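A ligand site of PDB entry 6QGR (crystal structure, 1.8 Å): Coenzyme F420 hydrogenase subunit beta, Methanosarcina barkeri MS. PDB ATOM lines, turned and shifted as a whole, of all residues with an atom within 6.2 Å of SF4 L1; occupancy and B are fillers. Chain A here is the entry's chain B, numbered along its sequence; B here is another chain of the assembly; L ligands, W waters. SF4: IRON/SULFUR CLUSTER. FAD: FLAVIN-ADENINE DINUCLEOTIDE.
FE4 of SF4 L1 is bound by SG of Cys 138 (2.2 Å).
The side-chain sulfur of Cys 197 binds an iron atom (FE3) of SF4 L1.
N of Cys 108 sits close to S3 of SF4 L1, at 3.3 Å.
SG of Cys 108 binds FE1 of SF4 L1 (2.3 Å).
An iron atom (FE2) of SF4 L1 is bound by the side-chain sulfur of Cys 200, 2.3 Å away.
A sulfur (S1) of SF4 L1 lies close to the side-chain amino group (NZ) of Lys 266 (3.2 Å).
The backbone NH (N) of Cys 107 lies close to a sulfur (S3) of SF4 L1 (3.3 Å).
A sulfur (S4) of SF4 L1 lies close to the guanidinium group (NH2) of Arg 229 of chain B (3.4 Å).
The backbone NH (N) of Met 139 lies within hydrogen-bond range of a nitrogen (N5) of FAD L2, at 3.4 Å.
NZ of Lys 266 sits at hydrogen-bond distance from O of Cys 138.
The backbone carbonyl oxygen of Cys 197 lies within hydrogen-bond range of the side-chain amide nitrogen of Asn 270 (3.4 Å).
The side-chain sulfur (SG) of Cys 200 sits close to the side-chain amino group (NZ) of Lys 266, 3.4 Å away.
The backbone carbonyl oxygen (O) of Asp 202 is in hydrogen-bond range of the side-chain sulfur (SG) of Cys 107, at 3.4 Å.
The side-chain sulfur (SG) of Cys 107 lies within hydrogen-bond range of the backbone carbonyl oxygen (O) of Leu 136 (3.6 Å).
The guanidinium group (NH1) of Arg 229 of chain B sits at hydrogen-bond distance from the backbone carbonyl oxygen (O) of Gly 196, 2.8 Å away.
The backbone carbonyl oxygen of Asn 141 sits at hydrogen-bond distance from the backbone NH of Gln 194 (2.8 Å).
The side-chain amide nitrogen of Gln 194 lies within hydrogen-bond range of the backbone carbonyl oxygen of Met 189 of chain B, 3.4 Å away.
A sulfur (S1) of SF4 L1 sits close to the backbone carbonyl oxygen of Met 139, at 3.4 Å.
Glu 140 touches SF4 L1.
Asn 141 touches SF4 L1.
Met 189 of chain B touches SF4 L1 (CB to S4, 3.7 Å).
Hydrophobic or aromatic side chains within 4 Å of SF4 L1: Met 189 of chain B.
11 residues have an atom within 4 Å of SF4 L1: Cys 107, Cys 108, Cys 138, Met 139, Glu 140, Asn 141, Cys 197, Cys 200, Lys 266, Met 189 of chain B and Arg 229 of chain B.
Along chain A the residues within 4 Å of SF4 L1 span positions 107 to 266.
The nearest printed residue that does not touch SF4 L1 is Val 106 (4.04 Å).
Water W1 lies within hydrogen-bond range of a sulfur (S2) of SF4 L1 (3.1 Å) and the side-chain amide nitrogen (ND2) of Asn 141 (3.1 Å).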
ATOM      1  N   VAL A 106     -12.287 -33.708  18.196  1.00  0.00           N
ATOM      2  CA  VAL A 106     -12.017 -32.387  18.764  1.00  0.00           C
ATOM      3  C   VAL A 106     -13.151 -31.428  18.406  1.00  0.00           C
ATOM      4  O   VAL A 106     -14.135 -31.815  17.753  1.00  0.00           O
ATOM      5  CB  VAL A 106     -10.645 -31.870  18.298  1.00  0.00           C
ATOM      6  CG1 VAL A 106      -9.542 -32.654  19.017  1.00  0.00           C
ATOM      7  CG2 VAL A 106     -10.509 -32.008  16.808  1.00  0.00           C
ATOM      8  N   CYS A 107     -13.021 -30.154  18.810  1.00  0.00           N
ATOM      9  CA  CYS A 107     -14.189 -29.260  18.842  1.00  0.00           C
ATOM     10  C   CYS A 107     -14.832 -29.101  17.467  1.00  0.00           C
ATOM     11  O   CYS A 107     -16.058 -29.175  17.349  1.00  0.00           O
ATOM     12  CB  CYS A 107     -13.797 -27.903  19.427  1.00  0.00           C
ATOM     13  SG  CYS A 107     -12.769 -28.009  20.903  1.00  0.00           S
ATOM     14  N   CYS A 108     -14.010 -28.887  16.407  1.00  0.00           N
ATOM     15  CA  CYS A 108     -14.558 -28.705  15.057  1.00  0.00           C
ATOM     16  C   CYS A 108     -15.263 -29.955  14.539  1.00  0.00           C
ATOM     17  O   CYS A 108     -16.138 -29.849  13.669  1.00  0.00           O
ATOM     18  CB  CYS A 108     -13.445 -28.330  14.083  1.00  0.00           C
ATOM     19  SG  CYS A 108     -12.050 -29.496  14.172  1.00  0.00           S
ATOM     20  N   GLN A 109     -14.882 -31.117  15.074  1.00  0.00           N
ATOM     21  CA  GLN A 109     -15.509 -32.366  14.648  1.00  0.00           C
ATOM     22  C   GLN A 109     -16.861 -32.542  15.314  1.00  0.00           C
ATOM     23  O   GLN A 109     -17.812 -33.042  14.687  1.00  0.00           O
ATOM     24  CB  GLN A 109     -14.535 -33.530  14.925  1.00  0.00           C
ATOM     25  CG  GLN A 109     -13.381 -33.491  13.893  1.00  0.00           C
ATOM     26  CD  GLN A 109     -12.144 -34.263  14.302  1.00  0.00           C
ATOM     27  OE1 GLN A 109     -12.101 -34.890  15.384  1.00  0.00           O
ATOM     28  NE2 GLN A 109     -11.103 -34.202  13.459  1.00  0.00           N
ATOM     29  N   LEU A 136     -13.063 -33.678  22.654  1.00  0.00           N
ATOM     30  CA  LEU A 136     -11.804 -33.382  23.345  1.00  0.00           C
ATOM     31  C   LEU A 136     -11.577 -31.869  23.353  1.00  0.00           C
ATOM     32  O   LEU A 136     -11.931 -31.179  22.392  1.00  0.00           O
ATOM     33  CB  LEU A 136     -10.595 -34.051  22.670  1.00  0.00           C
ATOM     34  CG  LEU A 136     -10.633 -35.521  22.217  1.00  0.00           C
ATOM     35  CD1 LEU A 136      -9.263 -35.930  21.628  1.00  0.00           C
ATOM     36  CD2 LEU A 136     -11.060 -36.460  23.306  1.00  0.00           C
ATOM     37  N   CYS A 138      -9.243 -28.743  22.655  1.00  0.00           N
ATOM     38  CA  CYS A 138      -8.250 -28.631  21.588  1.00  0.00           C
ATOM     39  C   CYS A 138      -7.898 -27.167  21.402  1.00  0.00           C
ATOM     40  O   CYS A 138      -8.774 -26.375  21.040  1.00  0.00           O
ATOM     41  CB  CYS A 138      -8.782 -29.245  20.265  1.00  0.00           C
ATOM     42  SG  CYS A 138      -7.614 -29.073  18.902  1.00  0.00           S
ATOM     43  N   MET A 139      -6.614 -26.819  21.647  1.00  0.00           N
ATOM     44  CA  MET A 139      -6.127 -25.466  21.420  1.00  0.00           C
ATOM     45  C   MET A 139      -5.711 -25.263  19.977  1.00  0.00           C
ATOM     46  O   MET A 139      -6.011 -24.211  19.392  1.00  0.00           O
ATOM     47  CB  MET A 139      -4.957 -25.142  22.367  1.00  0.00           C
ATOM     48  CG  MET A 139      -4.454 -23.694  22.244  1.00  0.00           C
ATOM     49  SD  MET A 139      -5.692 -22.437  22.761  1.00  0.00           S
ATOM     50  CE  MET A 139      -5.659 -22.642  24.528  1.00  0.00           C
ATOM     51  N   GLU A 140      -5.045 -26.277  19.370  1.00  0.00           N
ATOM     52  CA  GLU A 140      -4.657 -26.226  17.954  1.00  0.00           C
ATOM     53  C   GLU A 140      -4.114 -27.591  17.495  1.00  0.00           C
ATOM     54  O   GLU A 140      -3.783 -28.457  18.303  1.00  0.00           O
ATOM     55  CB  GLU A 140      -3.620 -25.105  17.680  1.00  0.00           C
ATOM     56  CG  GLU A 140      -2.206 -25.394  18.253  1.00  0.00           C
ATOM     57  CD  GLU A 140      -1.976 -24.776  19.633  1.00  0.00           C
ATOM     58  OE1 GLU A 140      -2.255 -23.552  19.775  1.00  0.00           O
ATOM     59  OE2 GLU A 140      -1.534 -25.524  20.570  1.00  0.00           O
ATOM     60  N   ASN A 141      -4.061 -27.777  16.163  1.00  0.00           N
ATOM     61  CA  ASN A 141      -3.587 -29.033  15.580  1.00  0.00           C
ATOM     62  C   ASN A 141      -2.517 -28.745  14.509  1.00  0.00           C
ATOM     63  O   ASN A 141      -2.235 -27.584  14.158  1.00  0.00           O
ATOM     64  CB  ASN A 141      -4.769 -29.865  15.005  1.00  0.00           C
ATOM     65  CG  ASN A 141      -4.521 -31.372  15.084  1.00  0.00           C
ATOM     66  OD1 ASN A 141      -3.389 -31.804  15.358  1.00  0.00           O
ATOM     67  ND2 ASN A 141      -5.569 -32.187  14.848  1.00  0.00           N
ATOM     68  N   GLN A 194      -1.817 -25.872  11.944  1.00  0.00           N
ATOM     69  CA  GLN A 194      -2.708 -25.890  10.796  1.00  0.00           C
ATOM     70  C   GLN A 194      -3.426 -24.541  10.680  1.00  0.00           C
ATOM     71  O   GLN A 194      -4.126 -24.127  11.636  1.00  0.00           O
ATOM     72  CB  GLN A 194      -3.728 -27.063  10.934  1.00  0.00           C
ATOM     73  CG  GLN A 194      -4.882 -26.908   9.958  1.00  0.00           C
ATOM     74  CD  GLN A 194      -5.906 -28.075   9.959  1.00  0.00           C
ATOM     75  OE1 GLN A 194      -6.255 -28.588   8.889  1.00  0.00           O
ATOM     76  NE2 GLN A 194      -6.439 -28.425  11.140  1.00  0.00           N
ATOM     77  N   GLY A 196      -6.185 -23.388   9.365  1.00  0.00           N
ATOM     78  CA  GLY A 196      -7.623 -23.375   9.606  1.00  0.00           C
ATOM     79  C   GLY A 196      -8.013 -23.386  11.082  1.00  0.00           C
ATOM     80  O   GLY A 196      -9.188 -23.136  11.410  1.00  0.00           O
ATOM     81  N   CYS A 197      -7.078 -23.694  11.979  1.00  0.00           N
ATOM     82  CA  CYS A 197      -7.284 -23.629  13.418  1.00  0.00           C
ATOM     83  C   CYS A 197      -7.369 -22.181  13.932  1.00  0.00           C
ATOM     84  O   CYS A 197      -7.767 -21.946  15.080  1.00  0.00           O
ATOM     85  CB  CYS A 197      -6.151 -24.336  14.143  1.00  0.00           C
ATOM     86  SG  CYS A 197      -6.123 -26.131  13.943  1.00  0.00           S
ATOM     87  N   HIS A 198      -7.001 -21.213  13.102  1.00  0.00           N
ATOM     88  CA  HIS A 198      -6.832 -19.843  13.552  1.00  0.00           C
ATOM     89  C   HIS A 198      -8.139 -19.040  13.525  1.00  0.00           C
ATOM     90  O   HIS A 198      -8.161 -17.909  14.038  1.00  0.00           O
ATOM     91  CB  HIS A 198      -5.729 -19.207  12.735  1.00  0.00           C
ATOM     92  CG  HIS A 198      -4.391 -19.826  12.997  1.00  0.00           C
ATOM     93  ND1 HIS A 198      -3.329 -19.750  12.122  1.00  0.00           N
ATOM     94  CD2 HIS A 198      -3.952 -20.559  14.062  1.00  0.00           C
ATOM     95  CE1 HIS A 198      -2.292 -20.384  12.633  1.00  0.00           C
ATOM     96  NE2 HIS A 198      -2.639 -20.877  13.813  1.00  0.00           N
ATOM     97  N   CYS A 200     -10.877 -20.791  14.802  1.00  0.00           N
ATOM     98  CA  CYS A 200     -11.662 -21.668  15.667  1.00  0.00           C
ATOM     99  C   CYS A 200     -12.007 -20.949  16.987  1.00  0.00           C
ATOM    100  O   CYS A 200     -11.114 -20.493  17.702  1.00  0.00           O
ATOM    101  CB  CYS A 200     -10.876 -22.949  15.963  1.00  0.00           C
ATOM    102  SG  CYS A 200     -11.767 -24.100  16.966  1.00  0.00           S
ATOM    103  N   LEU A 201     -13.291 -20.939  17.338  1.00  0.00           N
ATOM    104  CA  LEU A 201     -13.816 -20.129  18.444  1.00  0.00           C
ATOM    105  C   LEU A 201     -14.383 -21.008  19.546  1.00  0.00           C
ATOM    106  O   LEU A 201     -15.378 -20.643  20.204  1.00  0.00           O
ATOM    107  CB  LEU A 201     -14.871 -19.164  17.910  1.00  0.00           C
ATOM    108  CG  LEU A 201     -14.401 -18.267  16.740  1.00  0.00           C
ATOM    109  CD1 LEU A 201     -15.555 -17.422  16.157  1.00  0.00           C
ATOM    110  CD2 LEU A 201     -13.231 -17.389  17.129  1.00  0.00           C
ATOM    111  N   ASP A 202     -13.770 -22.168  19.760  1.00  0.00           N
ATOM    112  CA  ASP A 202     -14.352 -23.242  20.552  1.00  0.00           C
ATOM    113  C   ASP A 202     -13.207 -24.024  21.187  1.00  0.00           C
ATOM    114  O   ASP A 202     -12.416 -24.655  20.489  1.00  0.00           O
ATOM    115  CB  ASP A 202     -15.212 -24.144  19.657  1.00  0.00           C
ATOM    116  CG  ASP A 202     -16.089 -25.130  20.440  1.00  0.00           C
ATOM    117  OD1 ASP A 202     -15.752 -25.564  21.563  1.00  0.00           O
ATOM    118  OD2 ASP A 202     -17.153 -25.480  19.922  1.00  0.00           O
ATOM    119  N   LYS A 266      -7.915 -18.171  23.666  1.00  0.00           N
ATOM    120  CA  LYS A 266      -8.164 -18.792  22.365  1.00  0.00           C
ATOM    121  C   LYS A 266      -9.217 -17.996  21.593  1.00  0.00           C
ATOM    122  O   LYS A 266      -8.957 -17.519  20.470  1.00  0.00           O
ATOM    123  CB  LYS A 266      -8.579 -20.272  22.500  1.00  0.00           C
ATOM    124  CG  LYS A 266      -8.678 -20.959  21.089  1.00  0.00           C
ATOM    125  CD  LYS A 266      -9.354 -22.315  21.057  1.00  0.00           C
ATOM    126  CE  LYS A 266      -9.292 -22.972  19.619  1.00  0.00           C
ATOM    127  NZ  LYS A 266      -9.649 -24.434  19.631  1.00  0.00           N
ATOM    128  N   ASN A 270      -8.528 -15.738  18.215  1.00  0.00           N
ATOM    129  CA  ASN A 270      -9.052 -16.214  16.933  1.00  0.00           C
ATOM    130  C   ASN A 270     -10.173 -15.326  16.421  1.00  0.00           C
ATOM    131  O   ASN A 270     -10.318 -15.168  15.205  1.00  0.00           O
ATOM    132  CB  ASN A 270      -9.504 -17.677  17.070  1.00  0.00           C
ATOM    133  CG  ASN A 270      -8.326 -18.626  17.266  1.00  0.00           C
ATOM    134  OD1 ASN A 270      -7.172 -18.223  17.109  1.00  0.00           O
ATOM    135  ND2 ASN A 270      -8.597 -19.890  17.607  1.00  0.00           N
ATOM    136  N   MET B 189     -10.094 -27.386   7.990  1.00  0.00           N
ATOM    137  CA  MET B 189      -9.440 -27.934   9.184  1.00  0.00           C
ATOM    138  C   MET B 189      -9.462 -29.458   9.222  1.00  0.00           C
ATOM    139  O   MET B 189      -9.305 -30.050  10.312  1.00  0.00           O
ATOM    140  CB  MET B 189     -10.055 -27.360  10.490  1.00  0.00           C
ATOM    141  CG  MET B 189     -11.560 -27.204  10.500  1.00  0.00           C
ATOM    142  SD  MET B 189     -12.438 -28.815  10.387  1.00  0.00           S
ATOM    143  CE  MET B 189     -14.116 -28.284   9.967  1.00  0.00           C
ATOM    144  N   ARG B 229     -17.217 -25.368   7.317  1.00  0.00           N
ATOM    145  CA  ARG B 229     -16.568 -24.081   7.047  1.00  0.00           C
ATOM    146  C   ARG B 229     -17.128 -23.414   5.792  1.00  0.00           C
ATOM    147  O   ARG B 229     -16.549 -22.431   5.305  1.00  0.00           O
ATOM    148  CB  ARG B 229     -15.034 -24.291   6.983  1.00  0.00           C
ATOM    149  CG  ARG B 229     -14.463 -24.761   8.374  1.00  0.00           C
ATOM    150  CD  ARG B 229     -14.435 -23.613   9.418  1.00  0.00           C
ATOM    151  NE  ARG B 229     -13.868 -23.921  10.768  1.00  0.00           N
ATOM    152  CZ  ARG B 229     -12.568 -23.859  11.084  1.00  0.00           C
ATOM    153  NH1 ARG B 229     -11.666 -23.553  10.168  1.00  0.00           N
ATOM    154  NH2 ARG B 229     -12.161 -24.087  12.320  1.00  0.00           N
HETATM  155 FE1  SF4 L   1     -10.330 -28.286  15.074  1.00  0.00          FE
HETATM  156 FE2  SF4 L   1     -10.360 -25.882  16.390  1.00  0.00          FE
HETATM  157 FE3  SF4 L   1      -8.096 -26.683  14.920  1.00  0.00          FE
HETATM  158 FE4  SF4 L   1      -8.658 -27.940  17.360  1.00  0.00          FE
HETATM  159  S1  SF4 L   1      -8.135 -25.661  17.126  1.00  0.00           S
HETATM  160  S2  SF4 L   1      -8.139 -29.032  15.245  1.00  0.00           S
HETATM  161  S3  SF4 L   1     -11.020 -27.951  17.382  1.00  0.00           S
HETATM  162  S4  SF4 L   1     -10.163 -26.196  13.994  1.00  0.00           S
HETATM  163  PA  FAD L   2      -7.867 -41.606  25.895  1.00  0.00           P
HETATM  164  O1A FAD L   2      -6.303 -41.661  25.891  1.00  0.00           O
HETATM  165  O2A FAD L   2      -8.554 -42.669  26.640  1.00  0.00           O
HETATM  166  O5B FAD L   2      -8.439 -41.756  24.346  1.00  0.00           O
HETATM  167  C5B FAD L   2      -7.958 -40.917  23.367  1.00  0.00           C
HETATM  168  C4B FAD L   2      -9.157 -40.290  22.626  1.00  0.00           C
HETATM  169  O4B FAD L   2      -8.651 -39.238  21.934  1.00  0.00           O
HETATM  170  C3B FAD L   2      -9.893 -41.267  21.656  1.00  0.00           C
HETATM  171  O3B FAD L   2     -11.261 -41.036  21.691  1.00  0.00           O
HETATM  172  C2B FAD L   2      -9.363 -40.757  20.294  1.00  0.00           C
HETATM  173  O2B FAD L   2     -10.335 -41.145  19.262  1.00  0.00           O
HETATM  174  C1B FAD L   2      -9.151 -39.358  20.441  1.00  0.00           C
HETATM  175  N9A FAD L   2      -8.152 -38.811  19.676  1.00  0.00           N
HETATM  176  C8A FAD L   2      -6.768 -39.027  19.856  1.00  0.00           C
HETATM  177  N7A FAD L   2      -6.115 -38.263  18.840  1.00  0.00           N
HETATM  178  C5A FAD L   2      -7.092 -37.625  18.079  1.00  0.00           C
HETATM  179  C6A FAD L   2      -7.001 -36.806  16.985  1.00  0.00           C
HETATM  180  N6A FAD L   2      -5.837 -36.315  16.289  1.00  0.00           N
HETATM  181  N1A FAD L   2      -8.063 -36.306  16.382  1.00  0.00           N
HETATM  182  C2A FAD L   2      -9.350 -36.588  16.844  1.00  0.00           C
HETATM  183  N3A FAD L   2      -9.509 -37.392  17.938  1.00  0.00           N
HETATM  184  C4A FAD L   2      -8.357 -37.965  18.594  1.00  0.00           C
HETATM  185  N1  FAD L   2      -6.681 -31.141  26.201  1.00  0.00           N
HETATM  186  C2  FAD L   2      -6.533 -29.963  27.085  1.00  0.00           C
HETATM  187  O2  FAD L   2      -6.864 -30.028  28.267  1.00  0.00           O
HETATM  188  N3  FAD L   2      -5.996 -28.749  26.477  1.00  0.00           N
HETATM  189  C4  FAD L   2      -5.583 -28.691  25.130  1.00  0.00           C
HETATM  190  O4  FAD L   2      -5.133 -27.697  24.653  1.00  0.00           O
HETATM  191  C4X FAD L   2      -5.721 -29.877  24.252  1.00  0.00           C
HETATM  192  N5  FAD L   2      -5.312 -29.755  22.812  1.00  0.00           N
HETATM  193  C5X FAD L   2      -5.536 -30.954  22.027  1.00  0.00           C
HETATM  194  C6  FAD L   2      -5.175 -30.890  20.657  1.00  0.00           C
HETATM  195  C7  FAD L   2      -5.381 -32.112  19.861  1.00  0.00           C
HETATM  196  C7M FAD L   2      -4.878 -31.714  18.406  1.00  0.00           C
HETATM  197  C8  FAD L   2      -5.952 -33.318  20.469  1.00  0.00           C
HETATM  198  C8M FAD L   2      -6.136 -34.498  19.525  1.00  0.00           C
HETATM  199  C9  FAD L   2      -6.317 -33.372  21.791  1.00  0.00           C
HETATM  200  C9A FAD L   2      -6.084 -32.163  22.592  1.00  0.00           C
HETATM  201  N10 FAD L   2      -6.462 -32.251  23.992  1.00  0.00           N
HETATM  202  C10 FAD L   2      -6.289 -31.066  24.791  1.00  0.00           C
HETATM  203  C1' FAD L   2      -7.095 -33.466  24.674  1.00  0.00           C
HETATM  204  C2' FAD L   2      -6.118 -34.282  25.444  1.00  0.00           C
HETATM  205  O2' FAD L   2      -4.807 -34.307  24.755  1.00  0.00           O
HETATM  206  C3' FAD L   2      -6.684 -35.698  25.498  1.00  0.00           C
HETATM  207  O3' FAD L   2      -6.900 -36.202  24.183  1.00  0.00           O
HETATM  208  C4' FAD L   2      -8.049 -35.650  26.226  1.00  0.00           C
HETATM  209  O4' FAD L   2      -7.828 -35.254  27.587  1.00  0.00           O
HETATM  210  C5' FAD L   2      -8.746 -37.021  26.174  1.00  0.00           C
HETATM  211  O5' FAD L   2      -7.888 -37.889  26.902  1.00  0.00           O
HETATM  212  P   FAD L   2      -8.360 -39.279  27.632  1.00  0.00           P
HETATM  213  O1P FAD L   2      -9.800 -39.171  28.143  1.00  0.00           O
HETATM  214  O2P FAD L   2      -7.476 -39.956  28.699  1.00  0.00           O
HETATM  215  O3P FAD L   2      -8.504 -40.236  26.299  1.00  0.00           O
HETATM  216  O   HOH W   1      -8.499 -31.740  13.797  1.00  0.00           O
